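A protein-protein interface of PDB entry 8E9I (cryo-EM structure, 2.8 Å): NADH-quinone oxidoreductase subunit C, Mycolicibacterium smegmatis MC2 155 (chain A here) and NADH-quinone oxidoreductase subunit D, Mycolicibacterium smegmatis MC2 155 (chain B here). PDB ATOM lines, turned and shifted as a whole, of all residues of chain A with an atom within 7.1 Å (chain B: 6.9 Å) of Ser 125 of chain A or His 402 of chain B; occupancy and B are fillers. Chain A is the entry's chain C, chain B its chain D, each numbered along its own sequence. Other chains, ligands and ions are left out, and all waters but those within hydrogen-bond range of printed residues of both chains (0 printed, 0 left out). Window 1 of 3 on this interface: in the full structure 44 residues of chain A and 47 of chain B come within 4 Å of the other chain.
O of Leu 122 of chain A sits at hydrogen-bond distance from NE of Arg 404 of chain B (2.5 Å). The backbone carbonyl oxygen of Gly 126 of chain A lies within hydrogen-bond range of the guanidinium group of Arg 400 of chain B (3.0 Å).
The backbone NH of Leu 122 of chain A sits at hydrogen-bond distance from the backbone carbonyl oxygen of Pro 142 of chain A, at 2.7 Å. O of Ser 125 of chain A lies within hydrogen-bond range of N of Val 140 of chain A, 2.9 Å away. O of His 138 of chain A lies within hydrogen-bond range of N of Val 127 of chain A (2.9 Å). The backbone NH (N) of Arg 404 of chain B lies within hydrogen-bond range of the backbone carbonyl oxygen (O) of Gly 387 of chain B (2.9 Å). The backbone NH (N) of His 389 of chain B is in hydrogen-bond range of the backbone carbonyl oxygen (O) of His 402 of chain B (2.9 Å). The backbone NH of Val 391 of chain B is in hydrogen-bond range of the backbone carbonyl oxygen of Arg 400 of chain B (2.9 Å).
Among the printed residues, pairs that only touch across the chains: Ser 125 of chain A with His 402 of chain B, Phe 186 of chain A with Arg 400 of chain B, Val 140 of chain A with His 389 of chain B, Val 124 of chain A with His 402 of chain B, Pro 142 of chain A with Tyr 376 of chain B, Leu 122 of chain A with Tyr 376 of chain B and Val 127 of chain A with Arg 400 of chain B.
Of the printed residues of chain B, Val 124 of chain A touches His 402 (3.7 Å). Printed residues of chain B within 4 Å of Ser 125 of chain A: His 402 (3.1 Å). Printed residues of chain B within 4 Å of Pro 142 of chain A: Tyr 376. Glu 82 of chain B touches none of the printed residues of chain A. Of the printed residues of chain A, His 389 of chain B touches Val 140 (3.7 Å). Met 390 of chain B touches none of the printed residues of chain A. Of the printed residues of chain A, Arg 400 of chain B touches Gly 126, Val 127 and Phe 186. Of chain A, only Val 124 and Ser 125 come within 4 Å of His 402 of chain B. The nearest residue of chain A that does not touch His 402 of chain B is His 178 of chain A (5.0 Å). The nearest printed residue of chain B that does not touch Val 140 of chain A is Tyr 376 of chain B (5.8 Å).
Of the 16 printed residues of chain B, 5 touch a printed residue of chain A. Hydrophobic or aromatic side chains of chain B that line the printed part of chain A: Tyr 376, His 389 and His 402. Printed residues of chain A that touch a printed residue of chain B: Leu 122, Val 124, Ser 125, Gly 126, Val 127, Val 140, Pro 142 and Phe 186. Hydrophobic or aromatic side chains of chain A that line the printed part of chain B: Leu 122, Val 127, Val 140, Pro 142 and Phe 186. Among the printed residues, no Asp or Glu carboxylate lies within 4 Å of a Lys or Arg side-chain nitrogen of the other chain.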
ATOM      1  N   LEU A 122      18.994  -1.859 -26.633  1.00  0.00           N
ATOM      2  CA  LEU A 122      18.053  -1.886 -25.527  1.00  0.00           C
ATOM      3  C   LEU A 122      18.707  -1.554 -24.198  1.00  0.00           C
ATOM      4  O   LEU A 122      17.999  -1.352 -23.206  1.00  0.00           O
ATOM      5  CB  LEU A 122      17.382  -3.255 -25.465  1.00  0.00           C
ATOM      6  CG  LEU A 122      16.475  -3.483 -26.673  1.00  0.00           C
ATOM      7  CD1 LEU A 122      16.510  -4.933 -27.093  1.00  0.00           C
ATOM      8  CD2 LEU A 122      15.059  -3.050 -26.379  1.00  0.00           C
ATOM      9  N   GLY A 123      20.031  -1.481 -24.152  1.00  0.00           N
ATOM     10  CA  GLY A 123      20.703  -1.077 -22.934  1.00  0.00           C
ATOM     11  C   GLY A 123      22.073  -1.712 -22.832  1.00  0.00           C
ATOM     12  O   GLY A 123      22.611  -2.223 -23.814  1.00  0.00           O
ATOM     13  N   VAL A 124      22.629  -1.651 -21.629  1.00  0.00           N
ATOM     14  CA  VAL A 124      23.912  -2.262 -21.310  1.00  0.00           C
ATOM     15  C   VAL A 124      23.789  -2.917 -19.947  1.00  0.00           C
ATOM     16  O   VAL A 124      23.276  -2.306 -19.004  1.00  0.00           O
ATOM     17  CB  VAL A 124      25.057  -1.237 -21.305  1.00  0.00           C
ATOM     18  CG1 VAL A 124      26.397  -1.944 -21.241  1.00  0.00           C
ATOM     19  CG2 VAL A 124      24.968  -0.355 -22.529  1.00  0.00           C
ATOM     20  N   SER A 125      24.246  -4.156 -19.840  1.00  0.00           N
ATOM     21  CA  SER A 125      24.220  -4.882 -18.580  1.00  0.00           C
ATOM     22  C   SER A 125      25.616  -5.390 -18.261  1.00  0.00           C
ATOM     23  O   SER A 125      26.227  -6.086 -19.074  1.00  0.00           O
ATOM     24  CB  SER A 125      23.235  -6.049 -18.641  1.00  0.00           C
ATOM     25  N   GLY A 126      26.117  -5.042 -17.087  1.00  0.00           N
ATOM     26  CA  GLY A 126      27.370  -5.582 -16.624  1.00  0.00           C
ATOM     27  C   GLY A 126      27.166  -6.917 -15.935  1.00  0.00           C
ATOM     28  O   GLY A 126      26.140  -7.165 -15.310  1.00  0.00           O
ATOM     29  N   VAL A 127      28.148  -7.794 -16.084  1.00  0.00           N
ATOM     30  CA  VAL A 127      28.157  -9.073 -15.390  1.00  0.00           C
ATOM     31  C   VAL A 127      29.598  -9.396 -15.028  1.00  0.00           C
ATOM     32  O   VAL A 127      30.495  -9.326 -15.873  1.00  0.00           O
ATOM     33  CB  VAL A 127      27.517 -10.186 -16.241  1.00  0.00           C
ATOM     34  CG1 VAL A 127      28.259 -10.354 -17.532  1.00  0.00           C
ATOM     35  CG2 VAL A 127      27.479 -11.489 -15.476  1.00  0.00           C
ATOM     36  N   HIS A 138      32.065  -8.243 -18.078  1.00  0.00           N
ATOM     37  CA  HIS A 138      31.470  -8.330 -19.402  1.00  0.00           C
ATOM     38  C   HIS A 138      30.301  -7.364 -19.494  1.00  0.00           C
ATOM     39  O   HIS A 138      29.378  -7.420 -18.678  1.00  0.00           O
ATOM     40  CB  HIS A 138      30.989  -9.747 -19.706  1.00  0.00           C
ATOM     41  CG  HIS A 138      32.091 -10.751 -19.801  1.00  0.00           C
ATOM     42  ND1 HIS A 138      32.137 -11.714 -20.785  1.00  0.00           N
ATOM     43  CD2 HIS A 138      33.179 -10.953 -19.023  1.00  0.00           C
ATOM     44  CE1 HIS A 138      33.213 -12.461 -20.614  1.00  0.00           C
ATOM     45  NE2 HIS A 138      33.861 -12.021 -19.552  1.00  0.00           N
ATOM     46  N   ALA A 139      30.343  -6.489 -20.487  1.00  0.00           N
ATOM     47  CA  ALA A 139      29.214  -5.633 -20.805  1.00  0.00           C
ATOM     48  C   ALA A 139      28.439  -6.264 -21.949  1.00  0.00           C
ATOM     49  O   ALA A 139      29.020  -6.627 -22.974  1.00  0.00           O
ATOM     50  CB  ALA A 139      29.682  -4.232 -21.186  1.00  0.00           C
ATOM     51  N   VAL A 140      27.132  -6.397 -21.767  1.00  0.00           N
ATOM     52  CA  VAL A 140      26.249  -7.012 -22.744  1.00  0.00           C
ATOM     53  C   VAL A 140      25.350  -5.930 -23.315  1.00  0.00           C
ATOM     54  O   VAL A 140      24.742  -5.152 -22.566  1.00  0.00           O
ATOM     55  CB  VAL A 140      25.427  -8.150 -22.119  1.00  0.00           C
ATOM     56  CG1 VAL A 140      24.515  -8.777 -23.157  1.00  0.00           C
ATOM     57  CG2 VAL A 140      26.354  -9.190 -21.522  1.00  0.00           C
ATOM     58  N   TYR A 141      25.290  -5.871 -24.643  1.00  0.00           N
ATOM     59  CA  TYR A 141      24.506  -4.901 -25.396  1.00  0.00           C
ATOM     60  C   TYR A 141      23.446  -5.664 -26.170  1.00  0.00           C
ATOM     61  O   TYR A 141      23.754  -6.288 -27.192  1.00  0.00           O
ATOM     62  CB  TYR A 141      25.394  -4.112 -26.356  1.00  0.00           C
ATOM     63  CG  TYR A 141      26.393  -3.202 -25.702  1.00  0.00           C
ATOM     64  CD1 TYR A 141      27.619  -3.678 -25.278  1.00  0.00           C
ATOM     65  CD2 TYR A 141      26.123  -1.859 -25.537  1.00  0.00           C
ATOM     66  CE1 TYR A 141      28.541  -2.842 -24.699  1.00  0.00           C
ATOM     67  CE2 TYR A 141      27.038  -1.019 -24.958  1.00  0.00           C
ATOM     68  CZ  TYR A 141      28.245  -1.514 -24.541  1.00  0.00           C
ATOM     69  OH  TYR A 141      29.154  -0.666 -23.961  1.00  0.00           O
ATOM     70  N   PRO A 142      22.198  -5.680 -25.717  1.00  0.00           N
ATOM     71  CA  PRO A 142      21.129  -6.233 -26.555  1.00  0.00           C
ATOM     72  C   PRO A 142      20.733  -5.246 -27.640  1.00  0.00           C
ATOM     73  O   PRO A 142      20.289  -4.134 -27.349  1.00  0.00           O
ATOM     74  CB  PRO A 142      19.987  -6.468 -25.563  1.00  0.00           C
ATOM     75  CG  PRO A 142      20.260  -5.533 -24.462  1.00  0.00           C
ATOM     76  CD  PRO A 142      21.739  -5.422 -24.348  1.00  0.00           C
ATOM     77  N   LEU A 154      25.717  -8.132 -28.260  1.00  0.00           N
ATOM     78  CA  LEU A 154      27.159  -7.950 -28.213  1.00  0.00           C
ATOM     79  C   LEU A 154      27.656  -8.176 -26.795  1.00  0.00           C
ATOM     80  O   LEU A 154      26.968  -7.874 -25.820  1.00  0.00           O
ATOM     81  CB  LEU A 154      27.553  -6.550 -28.672  1.00  0.00           C
ATOM     82  CG  LEU A 154      26.839  -6.054 -29.921  1.00  0.00           C
ATOM     83  CD1 LEU A 154      27.369  -4.700 -30.333  1.00  0.00           C
ATOM     84  CD2 LEU A 154      27.002  -7.060 -31.039  1.00  0.00           C
ATOM     85  N   HIS A 178      22.451   3.502 -19.122  1.00  0.00           N
ATOM     86  CA  HIS A 178      22.844   2.128 -18.852  1.00  0.00           C
ATOM     87  C   HIS A 178      24.330   2.054 -18.555  1.00  0.00           C
ATOM     88  O   HIS A 178      24.735   1.568 -17.492  1.00  0.00           O
ATOM     89  CB  HIS A 178      22.482   1.239 -20.033  1.00  0.00           C
ATOM     90  CG  HIS A 178      21.012   1.164 -20.292  1.00  0.00           C
ATOM     91  ND1 HIS A 178      20.188   0.269 -19.648  1.00  0.00           N
ATOM     92  CD2 HIS A 178      20.216   1.885 -21.115  1.00  0.00           C
ATOM     93  CE1 HIS A 178      18.947   0.437 -20.068  1.00  0.00           C
ATOM     94  NE2 HIS A 178      18.938   1.410 -20.961  1.00  0.00           N
ATOM     95  N   GLU A 179      25.151   2.604 -19.446  1.00  0.00           N
ATOM     96  CA  GLU A 179      26.580   2.642 -19.193  1.00  0.00           C
ATOM     97  C   GLU A 179      26.878   3.256 -17.837  1.00  0.00           C
ATOM     98  O   GLU A 179      27.813   2.827 -17.156  1.00  0.00           O
ATOM     99  CB  GLU A 179      27.291   3.421 -20.297  1.00  0.00           C
ATOM    100  N   GLU A 181      24.780   3.238 -15.061  1.00  0.00           N
ATOM    101  CA  GLU A 181      24.421   2.268 -14.038  1.00  0.00           C
ATOM    102  C   GLU A 181      25.452   1.155 -13.984  1.00  0.00           C
ATOM    103  O   GLU A 181      25.981   0.832 -12.916  1.00  0.00           O
ATOM    104  CB  GLU A 181      23.026   1.706 -14.307  1.00  0.00           C
ATOM    105  N   THR A 182      25.795   0.595 -15.145  1.00  0.00           N
ATOM    106  CA  THR A 182      26.791  -0.463 -15.177  1.00  0.00           C
ATOM    107  C   THR A 182      28.086  -0.026 -14.514  1.00  0.00           C
ATOM    108  O   THR A 182      28.679  -0.800 -13.757  1.00  0.00           O
ATOM    109  CB  THR A 182      27.065  -0.896 -16.611  1.00  0.00           C
ATOM    110  OG1 THR A 182      27.335   0.251 -17.415  1.00  0.00           O
ATOM    111  CG2 THR A 182      25.864  -1.610 -17.175  1.00  0.00           C
ATOM    112  N   PHE A 185      27.588   0.086 -10.770  1.00  0.00           N
ATOM    113  CA  PHE A 185      27.387  -1.229 -10.192  1.00  0.00           C
ATOM    114  C   PHE A 185      28.590  -2.135 -10.385  1.00  0.00           C
ATOM    115  O   PHE A 185      28.738  -3.117  -9.653  1.00  0.00           O
ATOM    116  CB  PHE A 185      26.147  -1.849 -10.823  1.00  0.00           C
ATOM    117  CG  PHE A 185      24.860  -1.261 -10.336  1.00  0.00           C
ATOM    118  CD1 PHE A 185      24.842  -0.319  -9.324  1.00  0.00           C
ATOM    119  CD2 PHE A 185      23.665  -1.624 -10.921  1.00  0.00           C
ATOM    120  CE1 PHE A 185      23.663   0.223  -8.888  1.00  0.00           C
ATOM    121  CE2 PHE A 185      22.481  -1.078 -10.491  1.00  0.00           C
ATOM    122  CZ  PHE A 185      22.483  -0.153  -9.471  1.00  0.00           C
ATOM    123  N   PHE A 186      29.461  -1.829 -11.348  1.00  0.00           N
ATOM    124  CA  PHE A 186      30.587  -2.699 -11.643  1.00  0.00           C
ATOM    125  C   PHE A 186      31.912  -1.977 -11.752  1.00  0.00           C
ATOM    126  O   PHE A 186      32.954  -2.628 -11.636  1.00  0.00           O
ATOM    127  CB  PHE A 186      30.345  -3.463 -12.951  1.00  0.00           C
ATOM    128  CG  PHE A 186      29.187  -4.404 -12.887  1.00  0.00           C
ATOM    129  CD1 PHE A 186      29.332  -5.658 -12.333  1.00  0.00           C
ATOM    130  CD2 PHE A 186      27.953  -4.033 -13.376  1.00  0.00           C
ATOM    131  CE1 PHE A 186      28.269  -6.524 -12.268  1.00  0.00           C
ATOM    132  CE2 PHE A 186      26.888  -4.897 -13.316  1.00  0.00           C
ATOM    133  CZ  PHE A 186      27.046  -6.144 -12.759  1.00  0.00           C
ATOM    134  N   ILE A 188      32.932  -0.606 -14.491  1.00  0.00           N
ATOM    135  CA  ILE A 188      33.350  -0.620 -15.884  1.00  0.00           C
ATOM    136  C   ILE A 188      33.422   0.819 -16.371  1.00  0.00           C
ATOM    137  O   ILE A 188      32.396   1.494 -16.506  1.00  0.00           O
ATOM    138  CB  ILE A 188      32.384  -1.451 -16.737  1.00  0.00           C
ATOM    139  CG1 ILE A 188      32.451  -2.924 -16.330  1.00  0.00           C
ATOM    140  CG2 ILE A 188      32.709  -1.293 -18.212  1.00  0.00           C
ATOM    141  CD1 ILE A 188      31.310  -3.763 -16.868  1.00  0.00           C
ATOM    142  N   PHE A 190      33.475   3.328 -18.906  1.00  0.00           N
ATOM    143  CA  PHE A 190      33.195   3.595 -20.312  1.00  0.00           C
ATOM    144  C   PHE A 190      33.882   4.901 -20.697  1.00  0.00           C
ATOM    145  O   PHE A 190      33.322   5.995 -20.603  1.00  0.00           O
ATOM    146  CB  PHE A 190      31.697   3.644 -20.560  1.00  0.00           C
ATOM    147  CG  PHE A 190      31.005   2.353 -20.269  1.00  0.00           C
ATOM    148  CD1 PHE A 190      30.917   1.369 -21.235  1.00  0.00           C
ATOM    149  CD2 PHE A 190      30.451   2.116 -19.030  1.00  0.00           C
ATOM    150  CE1 PHE A 190      30.284   0.181 -20.971  1.00  0.00           C
ATOM    151  CE2 PHE A 190      29.819   0.925 -18.764  1.00  0.00           C
ATOM    152  CZ  PHE A 190      29.733  -0.040 -19.736  1.00  0.00           C
ATOM    153  N   GLU B  82      18.774  -6.701  -7.827  1.00  0.00           N
ATOM    154  CA  GLU B  82      19.604  -7.420  -8.784  1.00  0.00           C
ATOM    155  C   GLU B  82      20.731  -8.167  -8.093  1.00  0.00           C
ATOM    156  O   GLU B  82      21.155  -9.224  -8.569  1.00  0.00           O
ATOM    157  CB  GLU B  82      20.165  -6.453  -9.822  1.00  0.00           C
ATOM    158  N   LEU B  85      19.078 -10.992  -5.341  1.00  0.00           N
ATOM    159  CA  LEU B  85      18.681 -12.203  -6.044  1.00  0.00           C
ATOM    160  C   LEU B  85      19.763 -13.264  -5.970  1.00  0.00           C
ATOM    161  O   LEU B  85      19.473 -14.445  -5.769  1.00  0.00           O
ATOM    162  CB  LEU B  85      18.396 -11.892  -7.512  1.00  0.00           C
ATOM    163  CG  LEU B  85      17.055 -11.253  -7.836  1.00  0.00           C
ATOM    164  CD1 LEU B  85      17.096 -10.608  -9.202  1.00  0.00           C
ATOM    165  CD2 LEU B  85      15.974 -12.301  -7.787  1.00  0.00           C
ATOM    166  N   MET B 100      10.222  -5.628  -8.382  1.00  0.00           N
ATOM    167  CA  MET B 100      10.923  -4.582  -9.118  1.00  0.00           C
ATOM    168  C   MET B 100       9.947  -3.594  -9.733  1.00  0.00           C
ATOM    169  O   MET B 100       9.868  -2.438  -9.309  1.00  0.00           O
ATOM    170  CB  MET B 100      11.801  -5.200 -10.205  1.00  0.00           C
ATOM    171  CG  MET B 100      12.959  -6.005  -9.672  1.00  0.00           C
ATOM    172  SD  MET B 100      13.949  -6.711 -10.985  1.00  0.00           S
ATOM    173  CE  MET B 100      15.135  -7.649 -10.046  1.00  0.00           C
ATOM    174  N   TYR B 376      19.121 -13.501 -23.003  1.00  0.00           N
ATOM    175  CA  TYR B 376      18.394 -12.246 -22.893  1.00  0.00           C
ATOM    176  C   TYR B 376      17.002 -12.472 -23.463  1.00  0.00           C
ATOM    177  O   TYR B 376      16.855 -12.776 -24.651  1.00  0.00           O
ATOM    178  CB  TYR B 376      19.113 -11.118 -23.622  1.00  0.00           C
ATOM    179  CG  TYR B 376      18.406  -9.799 -23.488  1.00  0.00           C
ATOM    180  CD1 TYR B 376      17.407  -9.436 -24.374  1.00  0.00           C
ATOM    181  CD2 TYR B 376      18.728  -8.922 -22.466  1.00  0.00           C
ATOM    182  CE1 TYR B 376      16.758  -8.237 -24.251  1.00  0.00           C
ATOM    183  CE2 TYR B 376      18.082  -7.722 -22.334  1.00  0.00           C
ATOM    184  CZ  TYR B 376      17.097  -7.383 -23.230  1.00  0.00           C
ATOM    185  OH  TYR B 376      16.443  -6.180 -23.112  1.00  0.00           O
ATOM    186  N   GLY B 387      13.230  -6.207 -20.716  1.00  0.00           N
ATOM    187  CA  GLY B 387      14.196  -7.245 -21.015  1.00  0.00           C
ATOM    188  C   GLY B 387      14.813  -7.798 -19.747  1.00  0.00           C
ATOM    189  O   GLY B 387      14.895  -7.110 -18.731  1.00  0.00           O
ATOM    190  N   VAL B 388      15.258  -9.046 -19.813  1.00  0.00           N
ATOM    191  CA  VAL B 388      15.890  -9.708 -18.687  1.00  0.00           C
ATOM    192  C   VAL B 388      17.127 -10.407 -19.218  1.00  0.00           C
ATOM    193  O   VAL B 388      17.024 -11.290 -20.077  1.00  0.00           O
ATOM    194  CB  VAL B 388      14.958 -10.709 -17.997  1.00  0.00           C
ATOM    195  CG1 VAL B 388      15.692 -11.433 -16.883  1.00  0.00           C
ATOM    196  CG2 VAL B 388      13.742  -9.994 -17.472  1.00  0.00           C
ATOM    197  N   HIS B 389      18.294  -9.985 -18.747  1.00  0.00           N
ATOM    198  CA  HIS B 389      19.525 -10.716 -18.977  1.00  0.00           C
ATOM    199  C   HIS B 389      19.759 -11.665 -17.816  1.00  0.00           C
ATOM    200  O   HIS B 389      19.883 -11.232 -16.668  1.00  0.00           O
ATOM    201  CB  HIS B 389      20.698  -9.757 -19.124  1.00  0.00           C
ATOM    202  CG  HIS B 389      21.994 -10.443 -19.402  1.00  0.00           C
ATOM    203  ND1 HIS B 389      22.157 -11.322 -20.448  1.00  0.00           N
ATOM    204  CD2 HIS B 389      23.188 -10.381 -18.771  1.00  0.00           C
ATOM    205  CE1 HIS B 389      23.397 -11.775 -20.448  1.00  0.00           C
ATOM    206  NE2 HIS B 389      24.044 -11.218 -19.441  1.00  0.00           N
ATOM    207  N   MET B 390      19.818 -12.955 -18.112  1.00  0.00           N
ATOM    208  CA  MET B 390      19.910 -13.979 -17.090  1.00  0.00           C
ATOM    209  C   MET B 390      21.158 -14.801 -17.346  1.00  0.00           C
ATOM    210  O   MET B 390      21.385 -15.264 -18.466  1.00  0.00           O
ATOM    211  CB  MET B 390      18.666 -14.868 -17.109  1.00  0.00           C
ATOM    212  CG  MET B 390      18.545 -15.801 -15.939  1.00  0.00           C
ATOM    213  SD  MET B 390      16.950 -16.624 -15.927  1.00  0.00           S
ATOM    214  CE  MET B 390      15.897 -15.276 -15.418  1.00  0.00           C
ATOM    215  N   VAL B 391      21.968 -14.967 -16.306  1.00  0.00           N
ATOM    216  CA  VAL B 391      23.210 -15.720 -16.373  1.00  0.00           C
ATOM    217  C   VAL B 391      23.187 -16.758 -15.267  1.00  0.00           C
ATOM    218  O   VAL B 391      22.917 -16.428 -14.106  1.00  0.00           O
ATOM    219  CB  VAL B 391      24.445 -14.818 -16.227  1.00  0.00           C
ATOM    220  CG1 VAL B 391      25.709 -15.618 -16.442  1.00  0.00           C
ATOM    221  CG2 VAL B 391      24.370 -13.653 -17.186  1.00  0.00           C
ATOM    222  N   ARG B 400      23.355 -14.077 -12.414  1.00  0.00           N
ATOM    223  CA  ARG B 400      23.051 -12.692 -12.731  1.00  0.00           C
ATOM    224  C   ARG B 400      21.620 -12.601 -13.222  1.00  0.00           C
ATOM    225  O   ARG B 400      21.187 -13.413 -14.037  1.00  0.00           O
ATOM    226  CB  ARG B 400      24.001 -12.150 -13.798  1.00  0.00           C
ATOM    227  CG  ARG B 400      23.826 -10.690 -14.150  1.00  0.00           C
ATOM    228  CD  ARG B 400      24.429  -9.783 -13.112  1.00  0.00           C
ATOM    229  NE  ARG B 400      24.162  -8.383 -13.420  1.00  0.00           N
ATOM    230  CZ  ARG B 400      23.466  -7.550 -12.660  1.00  0.00           C
ATOM    231  NH1 ARG B 400      22.916  -7.940 -11.523  1.00  0.00           N
ATOM    232  NH2 ARG B 400      23.320  -6.291 -13.052  1.00  0.00           N
ATOM    233  N   VAL B 401      20.893 -11.609 -12.723  1.00  0.00           N
ATOM    234  CA  VAL B 401      19.579 -11.285 -13.257  1.00  0.00           C
ATOM    235  C   VAL B 401      19.477  -9.775 -13.370  1.00  0.00           C
ATOM    236  O   VAL B 401      19.231  -9.082 -12.379  1.00  0.00           O
ATOM    237  CB  VAL B 401      18.455 -11.856 -12.379  1.00  0.00           C
ATOM    238  CG1 VAL B 401      17.107 -11.519 -12.970  1.00  0.00           C
ATOM    239  CG2 VAL B 401      18.610 -13.346 -12.238  1.00  0.00           C
ATOM    240  N   HIS B 402      19.676  -9.257 -14.572  1.00  0.00           N
ATOM    241  CA  HIS B 402      19.616  -7.829 -14.828  1.00  0.00           C
ATOM    242  C   HIS B 402      18.321  -7.510 -15.550  1.00  0.00           C
ATOM    243  O   HIS B 402      18.031  -8.100 -16.593  1.00  0.00           O
ATOM    244  CB  HIS B 402      20.811  -7.377 -15.662  1.00  0.00           C
ATOM    245  CG  HIS B 402      20.747  -5.942 -16.076  1.00  0.00           C
ATOM    246  ND1 HIS B 402      20.480  -5.550 -17.369  1.00  0.00           N
ATOM    247  CD2 HIS B 402      20.905  -4.802 -15.363  1.00  0.00           C
ATOM    248  CE1 HIS B 402      20.481  -4.232 -17.436  1.00  0.00           C
ATOM    249  NE2 HIS B 402      20.736  -3.754 -16.233  1.00  0.00           N
ATOM    250  N   TYR B 403      17.539  -6.590 -14.997  1.00  0.00           N
ATOM    251  CA  TYR B 403      16.314  -6.158 -15.653  1.00  0.00           C
ATOM    252  C   TYR B 403      16.570  -4.867 -16.407  1.00  0.00           C
ATOM    253  O   TYR B 403      16.854  -3.827 -15.807  1.00  0.00           O
ATOM    254  CB  TYR B 403      15.161  -5.972 -14.676  1.00  0.00           C
ATOM    255  CG  TYR B 403      14.474  -7.252 -14.317  1.00  0.00           C
ATOM    256  CD1 TYR B 403      15.089  -8.467 -14.521  1.00  0.00           C
ATOM    257  CD2 TYR B 403      13.155  -7.252 -13.910  1.00  0.00           C
ATOM    258  CE1 TYR B 403      14.455  -9.633 -14.227  1.00  0.00           C
ATOM    259  CE2 TYR B 403      12.509  -8.416 -13.621  1.00  0.00           C
ATOM    260  CZ  TYR B 403      13.165  -9.604 -13.790  1.00  0.00           C
ATOM    261  OH  TYR B 403      12.536 -10.781 -13.512  1.00  0.00           O
ATOM    262  N   ARG B 404      16.470  -4.947 -17.725  1.00  0.00           N
ATOM    263  CA  ARG B 404      16.281  -3.778 -18.566  1.00  0.00           C
ATOM    264  C   ARG B 404      14.812  -3.399 -18.431  1.00  0.00           C
ATOM    265  O   ARG B 404      13.953  -3.827 -19.204  1.00  0.00           O
ATOM    266  CB  ARG B 404      16.658  -4.090 -20.005  1.00  0.00           C
ATOM    267  CG  ARG B 404      16.748  -2.873 -20.882  1.00  0.00           C
ATOM    268  CD  ARG B 404      15.433  -2.551 -21.542  1.00  0.00           C
ATOM    269  NE  ARG B 404      15.588  -1.459 -22.492  1.00  0.00           N
ATOM    270  CZ  ARG B 404      14.585  -0.826 -23.078  1.00  0.00           C
ATOM    271  NH1 ARG B 404      13.328  -1.164 -22.853  1.00  0.00           N
ATOM    272  NH2 ARG B 404      14.849   0.176 -23.908  1.00  0.00           N
ATOM    273  N   ASP B 405      14.516  -2.634 -17.397  1.00  0.00           N
ATOM    274  CA  ASP B 405      13.151  -2.166 -17.197  1.00  0.00           C
ATOM    275  C   ASP B 405      12.836  -1.055 -18.189  1.00  0.00           C
ATOM    276  O   ASP B 405      13.640  -0.135 -18.353  1.00  0.00           O
ATOM    277  CB  ASP B 405      12.951  -1.659 -15.780  1.00  0.00           C
ATOM    278  CG  ASP B 405      11.499  -1.393 -15.469  1.00  0.00           C
ATOM    279  OD1 ASP B 405      10.975  -0.353 -15.914  1.00  0.00           O
ATOM    280  OD2 ASP B 405      10.868  -2.237 -14.802  1.00  0.00           O
ATOM    281  N   ARG B 442      15.214  -0.568  -9.302  1.00  0.00           N
ATOM    282  CA  ARG B 442      15.472  -1.978  -8.990  1.00  0.00           C
ATOM    283  C   ARG B 442      16.417  -2.187  -7.814  1.00  0.00           C
ATOM    284  O   ARG B 442      17.528  -2.692  -7.979  1.00  0.00           O
ATOM    285  CB  ARG B 442      16.043  -2.701 -10.211  1.00  0.00           C
ATOM    286  CG  ARG B 442      15.108  -2.764 -11.397  1.00  0.00           C
ATOM    287  CD  ARG B 442      15.877  -2.674 -12.695  1.00  0.00           C
ATOM    288  NE  ARG B 442      16.460  -1.348 -12.865  1.00  0.00           N
ATOM    289  CZ  ARG B 442      17.758  -1.077 -12.850  1.00  0.00           C
ATOM    290  NH1 ARG B 442      18.665  -2.022 -12.669  1.00  0.00           N
ATOM    291  NH2 ARG B 442      18.155   0.182 -13.011  1.00  0.00           N
ATOM    292  OXT ARG B 442      16.096  -1.873  -6.673  1.00  0.00           O
